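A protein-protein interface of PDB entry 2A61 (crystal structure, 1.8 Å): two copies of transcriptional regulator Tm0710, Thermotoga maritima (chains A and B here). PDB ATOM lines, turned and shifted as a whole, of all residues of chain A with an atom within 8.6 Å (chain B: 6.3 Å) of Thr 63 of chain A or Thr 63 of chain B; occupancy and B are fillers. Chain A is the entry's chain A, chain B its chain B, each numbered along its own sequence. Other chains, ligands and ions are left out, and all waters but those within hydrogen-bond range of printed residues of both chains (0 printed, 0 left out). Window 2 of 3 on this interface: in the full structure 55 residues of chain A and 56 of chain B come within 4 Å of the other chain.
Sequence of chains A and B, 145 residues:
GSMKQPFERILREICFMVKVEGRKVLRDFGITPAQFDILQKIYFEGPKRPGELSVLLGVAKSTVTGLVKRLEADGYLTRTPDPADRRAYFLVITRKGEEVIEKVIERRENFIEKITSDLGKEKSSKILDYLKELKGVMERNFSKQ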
ATOM      1  N   ALA A  34     -21.647   1.044  13.997  1.00  0.00           N
ATOM      2  CA  ALA A  34     -21.806  -0.241  13.358  1.00  0.00           C
ATOM      3  C   ALA A  34     -22.122  -0.077  11.879  1.00  0.00           C
ATOM      4  O   ALA A  34     -21.604  -0.832  11.046  1.00  0.00           O
ATOM      5  CB  ALA A  34     -22.885  -1.055  14.045  1.00  0.00           C
ATOM      6  N   GLN A  35     -22.947   0.916  11.542  1.00  0.00           N
ATOM      7  CA  GLN A  35     -23.195   1.219  10.136  1.00  0.00           C
ATOM      8  C   GLN A  35     -21.920   1.635   9.405  1.00  0.00           C
ATOM      9  O   GLN A  35     -21.714   1.245   8.260  1.00  0.00           O
ATOM     10  CB  GLN A  35     -24.221   2.312   9.984  1.00  0.00           C
ATOM     11  CG  GLN A  35     -25.702   1.908  10.256  1.00  0.00           C
ATOM     12  CD  GLN A  35     -26.632   3.086   9.932  1.00  0.00           C
ATOM     13  OE1 GLN A  35     -26.426   4.184  10.444  1.00  0.00           O
ATOM     14  NE2 GLN A  35     -27.648   2.863   9.060  1.00  0.00           N
ATOM     15  N   ILE A  38     -19.657  -1.381   8.608  1.00  0.00           N
ATOM     16  CA  ILE A  38     -20.113  -2.025   7.360  1.00  0.00           C
ATOM     17  C   ILE A  38     -19.634  -1.251   6.131  1.00  0.00           C
ATOM     18  O   ILE A  38     -19.105  -1.846   5.182  1.00  0.00           O
ATOM     19  CB  ILE A  38     -21.648  -2.133   7.288  1.00  0.00           C
ATOM     20  CG1 ILE A  38     -22.159  -3.097   8.379  1.00  0.00           C
ATOM     21  CG2 ILE A  38     -22.100  -2.475   5.883  1.00  0.00           C
ATOM     22  CD1 ILE A  38     -23.643  -3.015   8.560  1.00  0.00           C
ATOM     23  N   PRO A  50     -24.378 -10.719   3.229  1.00  0.00           N
ATOM     24  CA  PRO A  50     -24.945 -10.361   4.523  1.00  0.00           C
ATOM     25  C   PRO A  50     -24.389 -11.199   5.669  1.00  0.00           C
ATOM     26  O   PRO A  50     -24.157 -10.667   6.723  1.00  0.00           O
ATOM     27  CB  PRO A  50     -26.450 -10.619   4.337  1.00  0.00           C
ATOM     28  CG  PRO A  50     -26.671 -10.560   2.904  1.00  0.00           C
ATOM     29  CD  PRO A  50     -25.429 -11.093   2.252  1.00  0.00           C
ATOM     30  N   LEU A  53     -20.935  -9.764   6.754  1.00  0.00           N
ATOM     31  CA  LEU A  53     -21.131  -8.574   7.602  1.00  0.00           C
ATOM     32  C   LEU A  53     -21.497  -8.956   9.045  1.00  0.00           C
ATOM     33  O   LEU A  53     -21.034  -8.331   9.987  1.00  0.00           O
ATOM     34  CB  LEU A  53     -22.196  -7.648   6.996  1.00  0.00           C
ATOM     35  CG  LEU A  53     -21.862  -7.025   5.632  1.00  0.00           C
ATOM     36  CD1 LEU A  53     -23.072  -6.135   5.118  1.00  0.00           C
ATOM     37  CD2 LEU A  53     -20.586  -6.201   5.719  1.00  0.00           C
ATOM     38  N   SER A  54     -22.323  -9.990   9.198  1.00  0.00           N
ATOM     39  CA  SER A  54     -22.693 -10.536  10.512  1.00  0.00           C
ATOM     40  C   SER A  54     -21.443 -11.040  11.303  1.00  0.00           C
ATOM     41  O   SER A  54     -21.263 -10.751  12.496  1.00  0.00           O
ATOM     42  CB  SER A  54     -23.737 -11.656  10.301  1.00  0.00           C
ATOM     43  OG  SER A  54     -23.889 -12.362  11.487  1.00  0.00           O
ATOM     44  N   LEU A  57     -19.083  -7.834  12.163  1.00  0.00           N
ATOM     45  CA  LEU A  57     -19.555  -7.065  13.316  1.00  0.00           C
ATOM     46  C   LEU A  57     -19.648  -7.891  14.567  1.00  0.00           C
ATOM     47  O   LEU A  57     -19.456  -7.374  15.677  1.00  0.00           O
ATOM     48  CB  LEU A  57     -20.923  -6.438  13.048  1.00  0.00           C
ATOM     49  CG  LEU A  57     -20.977  -5.339  12.008  1.00  0.00           C
ATOM     50  CD1 LEU A  57     -22.432  -4.998  11.619  1.00  0.00           C
ATOM     51  CD2 LEU A  57     -20.229  -4.136  12.446  1.00  0.00           C
ATOM     52  N   GLY A  58     -19.921  -9.178  14.394  1.00  0.00           N
ATOM     53  CA  GLY A  58     -20.230 -10.063  15.529  1.00  0.00           C
ATOM     54  C   GLY A  58     -21.629  -9.889  16.080  1.00  0.00           C
ATOM     55  O   GLY A  58     -21.854 -10.034  17.304  1.00  0.00           O
ATOM     56  N   VAL A  59     -22.570  -9.574  15.180  1.00  0.00           N
ATOM     57  CA  VAL A  59     -23.994  -9.455  15.536  1.00  0.00           C
ATOM     58  C   VAL A  59     -24.854 -10.398  14.676  1.00  0.00           C
ATOM     59  O   VAL A  59     -24.467 -10.763  13.559  1.00  0.00           O
ATOM     60  CB  VAL A  59     -24.545  -7.977  15.437  1.00  0.00           C
ATOM     61  CG1 VAL A  59     -23.904  -7.043  16.536  1.00  0.00           C
ATOM     62  CG2 VAL A  59     -24.435  -7.387  14.006  1.00  0.00           C
ATOM     63  N   ALA A  60     -26.017 -10.768  15.198  1.00  0.00           N
ATOM     64  CA  ALA A  60     -27.007 -11.566  14.471  1.00  0.00           C
ATOM     65  C   ALA A  60     -27.396 -10.982  13.105  1.00  0.00           C
ATOM     66  O   ALA A  60     -27.255  -9.763  12.845  1.00  0.00           O
ATOM     67  CB  ALA A  60     -28.254 -11.770  15.343  1.00  0.00           C
ATOM     68  N   LYS A  61     -27.911 -11.853  12.235  1.00  0.00           N
ATOM     69  CA  LYS A  61     -28.295 -11.449  10.887  1.00  0.00           C
ATOM     70  C   LYS A  61     -29.408 -10.394  10.925  1.00  0.00           C
ATOM     71  O   LYS A  61     -29.424  -9.487  10.092  1.00  0.00           O
ATOM     72  CB  LYS A  61     -28.750 -12.670  10.063  1.00  0.00           C
ATOM     73  CG  LYS A  61     -27.693 -13.770   9.970  1.00  0.00           C
ATOM     74  CD  LYS A  61     -26.688 -13.587   8.822  1.00  0.00           C
ATOM     75  CE  LYS A  61     -25.558 -14.591   8.982  1.00  0.00           C
ATOM     76  NZ  LYS A  61     -26.095 -15.985   9.181  1.00  0.00           N
ATOM     77  N   SER A  62     -30.337 -10.523  11.887  1.00  0.00           N
ATOM     78  CA  SER A  62     -31.415  -9.539  12.085  1.00  0.00           C
ATOM     79  C   SER A  62     -30.897  -8.138  12.314  1.00  0.00           C
ATOM     80  O   SER A  62     -31.460  -7.184  11.786  1.00  0.00           O
ATOM     81  CB  SER A  62     -32.370  -9.914  13.242  1.00  0.00           C
ATOM     82  OG  SER A  62     -31.674 -10.265  14.435  1.00  0.00           O
ATOM     83  N   THR A  63     -29.829  -8.011  13.103  1.00  0.00           N
ATOM     84  CA  THR A  63     -29.227  -6.705  13.360  1.00  0.00           C
ATOM     85  C   THR A  63     -28.630  -6.132  12.059  1.00  0.00           C
ATOM     86  O   THR A  63     -28.870  -4.979  11.688  1.00  0.00           O
ATOM     87  CB  THR A  63     -28.121  -6.820  14.424  1.00  0.00           C
ATOM     88  OG1 THR A  63     -28.637  -7.392  15.623  1.00  0.00           O
ATOM     89  CG2 THR A  63     -27.515  -5.450  14.730  1.00  0.00           C
ATOM     90  N   VAL A  64     -27.851  -6.964  11.366  1.00  0.00           N
ATOM     91  CA  VAL A  64     -27.259  -6.578  10.093  1.00  0.00           C
ATOM     92  C   VAL A  64     -28.357  -6.074   9.139  1.00  0.00           C
ATOM     93  O   VAL A  64     -28.224  -5.049   8.531  1.00  0.00           O
ATOM     94  CB  VAL A  64     -26.532  -7.776   9.445  1.00  0.00           C
ATOM     95  CG1 VAL A  64     -26.053  -7.386   8.052  1.00  0.00           C
ATOM     96  CG2 VAL A  64     -25.394  -8.244  10.344  1.00  0.00           C
ATOM     97  N   THR A  65     -29.443  -6.821   9.024  1.00  0.00           N
ATOM     98  CA  THR A  65     -30.550  -6.457   8.156  1.00  0.00           C
ATOM     99  C   THR A  65     -31.033  -5.083   8.474  1.00  0.00           C
ATOM    100  O   THR A  65     -31.224  -4.302   7.574  1.00  0.00           O
ATOM    101  CB  THR A  65     -31.761  -7.440   8.241  1.00  0.00           C
ATOM    102  OG1 THR A  65     -31.308  -8.753   7.926  1.00  0.00           O
ATOM    103  CG2 THR A  65     -32.845  -7.044   7.236  1.00  0.00           C
ATOM    104  N   GLY A  66     -31.233  -4.769   9.758  1.00  0.00           N
ATOM    105  CA  GLY A  66     -31.671  -3.407  10.148  1.00  0.00           C
ATOM    106  C   GLY A  66     -30.702  -2.291   9.776  1.00  0.00           C
ATOM    107  O   GLY A  66     -31.112  -1.219   9.269  1.00  0.00           O
ATOM    108  N   LEU A  67     -29.412  -2.531  10.032  1.00  0.00           N
ATOM    109  CA  LEU A  67     -28.363  -1.596   9.675  1.00  0.00           C
ATOM    110  C   LEU A  67     -28.254  -1.330   8.168  1.00  0.00           C
ATOM    111  O   LEU A  67     -28.096  -0.200   7.769  1.00  0.00           O
ATOM    112  CB  LEU A  67     -26.980  -2.057  10.234  1.00  0.00           C
ATOM    113  CG  LEU A  67     -26.857  -2.306  11.758  1.00  0.00           C
ATOM    114  CD1 LEU A  67     -25.590  -3.089  12.087  1.00  0.00           C
ATOM    115  CD2 LEU A  67     -26.873  -0.939  12.530  1.00  0.00           C
ATOM    116  N   VAL A  68     -28.239  -2.405   7.369  1.00  0.00           N
ATOM    117  CA  VAL A  68     -28.076  -2.348   5.903  1.00  0.00           C
ATOM    118  C   VAL A  68     -29.313  -1.699   5.243  1.00  0.00           C
ATOM    119  O   VAL A  68     -29.188  -0.897   4.335  1.00  0.00           O
ATOM    120  CB  VAL A  68     -27.804  -3.758   5.370  1.00  0.00           C
ATOM    121  CG1 VAL A  68     -27.981  -3.829   3.852  1.00  0.00           C
ATOM    122  CG2 VAL A  68     -26.344  -4.219   5.811  1.00  0.00           C
ATOM    123  N   LYS A  69     -30.490  -2.067   5.712  1.00  0.00           N
ATOM    124  CA  LYS A  69     -31.768  -1.524   5.162  1.00  0.00           C
ATOM    125  C   LYS A  69     -31.816   0.005   5.189  1.00  0.00           C
ATOM    126  O   LYS A  69     -32.284   0.638   4.245  1.00  0.00           O
ATOM    127  CB  LYS A  69     -32.922  -2.094   5.986  1.00  0.00           C
ATOM    128  CG  LYS A  69     -34.303  -1.553   5.705  1.00  0.00           C
ATOM    129  CD  LYS A  69     -35.355  -2.288   6.548  1.00  0.00           C
ATOM    130  CE  LYS A  69     -35.183  -2.031   8.070  1.00  0.00           C
ATOM    131  NZ  LYS A  69     -36.130  -2.821   8.901  1.00  0.00           N
ATOM    132  N   ARG A  70     -31.323   0.589   6.284  1.00  0.00           N
ATOM    133  CA  ARG A  70     -31.243   2.059   6.415  1.00  0.00           C
ATOM    134  C   ARG A  70     -30.176   2.630   5.488  1.00  0.00           C
ATOM    135  O   ARG A  70     -30.374   3.647   4.867  1.00  0.00           O
ATOM    136  CB  ARG A  70     -30.845   2.441   7.817  1.00  0.00           C
ATOM    137  CG  ARG A  70     -31.973   2.639   8.803  1.00  0.00           C
ATOM    138  CD  ARG A  70     -31.286   3.296  10.067  1.00  0.00           C
ATOM    139  NE  ARG A  70     -30.909   2.206  10.932  1.00  0.00           N
ATOM    140  CZ  ARG A  70     -30.078   2.271  11.953  1.00  0.00           C
ATOM    141  NH1 ARG A  70     -29.457   3.396  12.269  1.00  0.00           N
ATOM    142  NH2 ARG A  70     -29.893   1.179  12.651  1.00  0.00           N
ATOM    143  N   LEU B  57     -21.654   0.966  20.281  1.00  0.00           N
ATOM    144  CA  LEU B  57     -21.789   0.045  19.130  1.00  0.00           C
ATOM    145  C   LEU B  57     -22.588   0.608  17.956  1.00  0.00           C
ATOM    146  O   LEU B  57     -22.309   0.272  16.784  1.00  0.00           O
ATOM    147  CB  LEU B  57     -22.333  -1.326  19.587  1.00  0.00           C
ATOM    148  CG  LEU B  57     -21.534  -2.188  20.579  1.00  0.00           C
ATOM    149  CD1 LEU B  57     -22.370  -3.358  21.058  1.00  0.00           C
ATOM    150  CD2 LEU B  57     -20.245  -2.734  19.995  1.00  0.00           C
ATOM    151  N   VAL B  59     -26.099   0.508  17.847  1.00  0.00           N
ATOM    152  CA  VAL B  59     -27.138  -0.517  17.612  1.00  0.00           C
ATOM    153  C   VAL B  59     -28.278  -0.290  18.591  1.00  0.00           C
ATOM    154  O   VAL B  59     -28.156   0.481  19.562  1.00  0.00           O
ATOM    155  CB  VAL B  59     -26.589  -1.976  17.787  1.00  0.00           C
ATOM    156  CG1 VAL B  59     -25.553  -2.270  16.723  1.00  0.00           C
ATOM    157  CG2 VAL B  59     -25.988  -2.195  19.226  1.00  0.00           C
ATOM    158  N   ALA B  60     -29.384  -0.965  18.340  1.00  0.00           N
ATOM    159  CA  ALA B  60     -30.554  -0.858  19.202  1.00  0.00           C
ATOM    160  C   ALA B  60     -30.290  -1.583  20.514  1.00  0.00           C
ATOM    161  O   ALA B  60     -29.470  -2.482  20.589  1.00  0.00           O
ATOM    162  CB  ALA B  60     -31.741  -1.450  18.501  1.00  0.00           C
ATOM    163  N   LYS B  61     -31.003  -1.186  21.557  1.00  0.00           N
ATOM    164  CA  LYS B  61     -30.912  -1.823  22.863  1.00  0.00           C
ATOM    165  C   LYS B  61     -31.096  -3.324  22.741  1.00  0.00           C
ATOM    166  O   LYS B  61     -30.372  -4.062  23.409  1.00  0.00           O
ATOM    167  CB  LYS B  61     -31.961  -1.220  23.821  1.00  0.00           C
ATOM    168  CG  LYS B  61     -31.828  -1.735  25.234  1.00  0.00           C
ATOM    169  CD  LYS B  61     -32.860  -1.062  26.173  1.00  0.00           C
ATOM    170  CE  LYS B  61     -32.931  -1.774  27.513  1.00  0.00           C
ATOM    171  NZ  LYS B  61     -31.751  -1.556  28.318  1.00  0.00           N
ATOM    172  N   SER B  62     -32.044  -3.770  21.891  1.00  0.00           N
ATOM    173  CA  SER B  62     -32.312  -5.198  21.701  1.00  0.00           C
ATOM    174  C   SER B  62     -31.070  -5.997  21.283  1.00  0.00           C
ATOM    175  O   SER B  62     -30.888  -7.132  21.744  1.00  0.00           O
ATOM    176  CB  SER B  62     -33.420  -5.468  20.687  1.00  0.00           C
ATOM    177  OG  SER B  62     -33.121  -4.885  19.436  1.00  0.00           O
ATOM    178  N   THR B  63     -30.254  -5.405  20.408  1.00  0.00           N
ATOM    179  CA  THR B  63     -28.943  -5.991  20.058  1.00  0.00           C
ATOM    180  C   THR B  63     -28.006  -6.036  21.254  1.00  0.00           C
ATOM    181  O   THR B  63     -27.377  -7.070  21.521  1.00  0.00           O
ATOM    182  CB  THR B  63     -28.254  -5.193  18.962  1.00  0.00           C
ATOM    183  OG1 THR B  63     -29.119  -5.156  17.823  1.00  0.00           O
ATOM    184  CG2 THR B  63     -26.882  -5.847  18.585  1.00  0.00           C
ATOM    185  N   VAL B  64     -27.905  -4.930  21.995  1.00  0.00           N
ATOM    186  CA  VAL B  64     -27.036  -4.923  23.187  1.00  0.00           C
ATOM    187  C   VAL B  64     -27.478  -5.979  24.207  1.00  0.00           C
ATOM    188  O   VAL B  64     -26.660  -6.749  24.744  1.00  0.00           O
ATOM    189  CB  VAL B  64     -26.984  -3.523  23.830  1.00  0.00           C
ATOM    190  CG1 VAL B  64     -26.171  -3.521  25.136  1.00  0.00           C
ATOM    191  CG2 VAL B  64     -26.437  -2.474  22.825  1.00  0.00           C
ATOM    192  N   THR B  65     -28.785  -6.032  24.456  1.00  0.00           N
ATOM    193  CA  THR B  65     -29.342  -7.001  25.357  1.00  0.00           C
ATOM    194  C   THR B  65     -28.958  -8.442  25.020  1.00  0.00           C
ATOM    195  O   THR B  65     -28.569  -9.194  25.916  1.00  0.00           O
ATOM    196  CB  THR B  65     -30.871  -6.876  25.421  1.00  0.00           C
ATOM    197  OG1 THR B  65     -31.185  -5.549  25.861  1.00  0.00           O
ATOM    198  CG2 THR B  65     -31.473  -7.924  26.406  1.00  0.00           C
ATOM    199  N   GLY B  66     -29.062  -8.812  23.740  1.00  0.00           N
ATOM    200  CA  GLY B  66     -28.635 -10.155  23.250  1.00  0.00           C
ATOM    201  C   GLY B  66     -27.151 -10.421  23.493  1.00  0.00           C
ATOM    202  O   GLY B  66     -26.789 -11.484  23.998  1.00  0.00           O
ATOM    203  N   LEU B  67     -26.301  -9.445  23.141  1.00  0.00           N
ATOM    204  CA  LEU B  67     -24.813  -9.538  23.339  1.00  0.00           C
ATOM    205  C   LEU B  67     -24.402  -9.655  24.788  1.00  0.00           C
ATOM    206  O   LEU B  67     -23.514 -10.456  25.146  1.00  0.00           O
ATOM    207  CB  LEU B  67     -24.100  -8.331  22.712  1.00  0.00           C
ATOM    208  CG  LEU B  67     -24.205  -8.137  21.167  1.00  0.00           C
ATOM    209  CD1 LEU B  67     -23.653  -6.755  20.809  1.00  0.00           C
ATOM    210  CD2 LEU B  67     -23.484  -9.251  20.420  1.00  0.00           C
ATOM    211  N   VAL B  68     -25.073  -8.883  25.644  1.00  0.00           N
ATOM    212  CA  VAL B  68     -24.794  -8.854  27.062  1.00  0.00           C
ATOM    213  C   VAL B  68     -25.287 -10.122  27.772  1.00  0.00           C
ATOM    214  O   VAL B  68     -24.583 -10.681  28.616  1.00  0.00           O
ATOM    215  CB  VAL B  68     -25.405  -7.580  27.736  1.00  0.00           C
ATOM    216  CG1 VAL B  68     -25.561  -7.780  29.277  1.00  0.00           C
ATOM    217  CG2 VAL B  68     -24.555  -6.355  27.417  1.00  0.00           C
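Hydrophobic or aromatic side chains of chain B within 4 Å of the printed part of chain A: Val 59 and Leu 67.
N of Ala 34 of chain A sits at hydrogen-bond distance from O of Leu 57 of chain B (3.0 Å).
The side-chain hydroxyl of Thr 63 of chain A lies within hydrogen-bond range of the side-chain hydroxyl of Thr 63 of chain B (3.2 Å).
Val 59 of chain A touches Thr 63 of chain B, but with the chains exchanged Thr 63 of chain A does not touch Val 59 of chain B (4.2 Å).
Thr 63 of chain B touches its own counterpart, Thr 63 of chain A.
Positions printed for both chains: 57, 59, 60, 61, 62, 63, 64, 65, 66, 67 and 68.
Of the 5 pairs that touch across the chains among the printed residues, 1 has its exchanged pair printed and touching as well.
Among the printed residues, pairs that only touch across the chains: Gly 58 of chain A with Leu 67 of chain B, Val 59 of chain A with Thr 63 of chain B and Ala 34 of chain A with Val 59 of chain B.
The side-chain hydroxyl (OG) of Ser 54 of chain A sits at hydrogen-bond distance from the backbone carbonyl oxygen (O) of Val 59 of chain A, 2.7 Å away.
Of the printed residues of chain B, Ala 34 of chain A touches Leu 57 and Val 59.
Ser 54 of chain A touches none of the printed residues of chain B.
Printed residues of chain B within 4 Å of Val 59 of chain A: Thr 63 (3.8 Å).
Thr 63 of chain A touches one residue of chain B.
Printed residues of chain A within 4 Å of Leu 57 of chain B: Ala 34 (3.0 Å).
Of the printed residues of chain A, Val 59 of chain B touches Ala 34 (3.97 Å).
No residue of chain A comes within 4 Å of Ser 62 of chain B.
Thr 63 of chain B touches just these residues of chain A: Val 59 and Thr 63.
Printed residues of chain A within 4 Å of Leu 67 of chain B: Gly 58 (3.6 Å).
Val 68 of chain B touches none of the printed residues of chain A.
The nearest residue of chain B that does not touch Thr 63 of chain A is Val 59 of chain B (4.2 Å).
The nearest printed residue of chain A that does not touch Leu 67 of chain B is Val 59 of chain A (4.3 Å).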
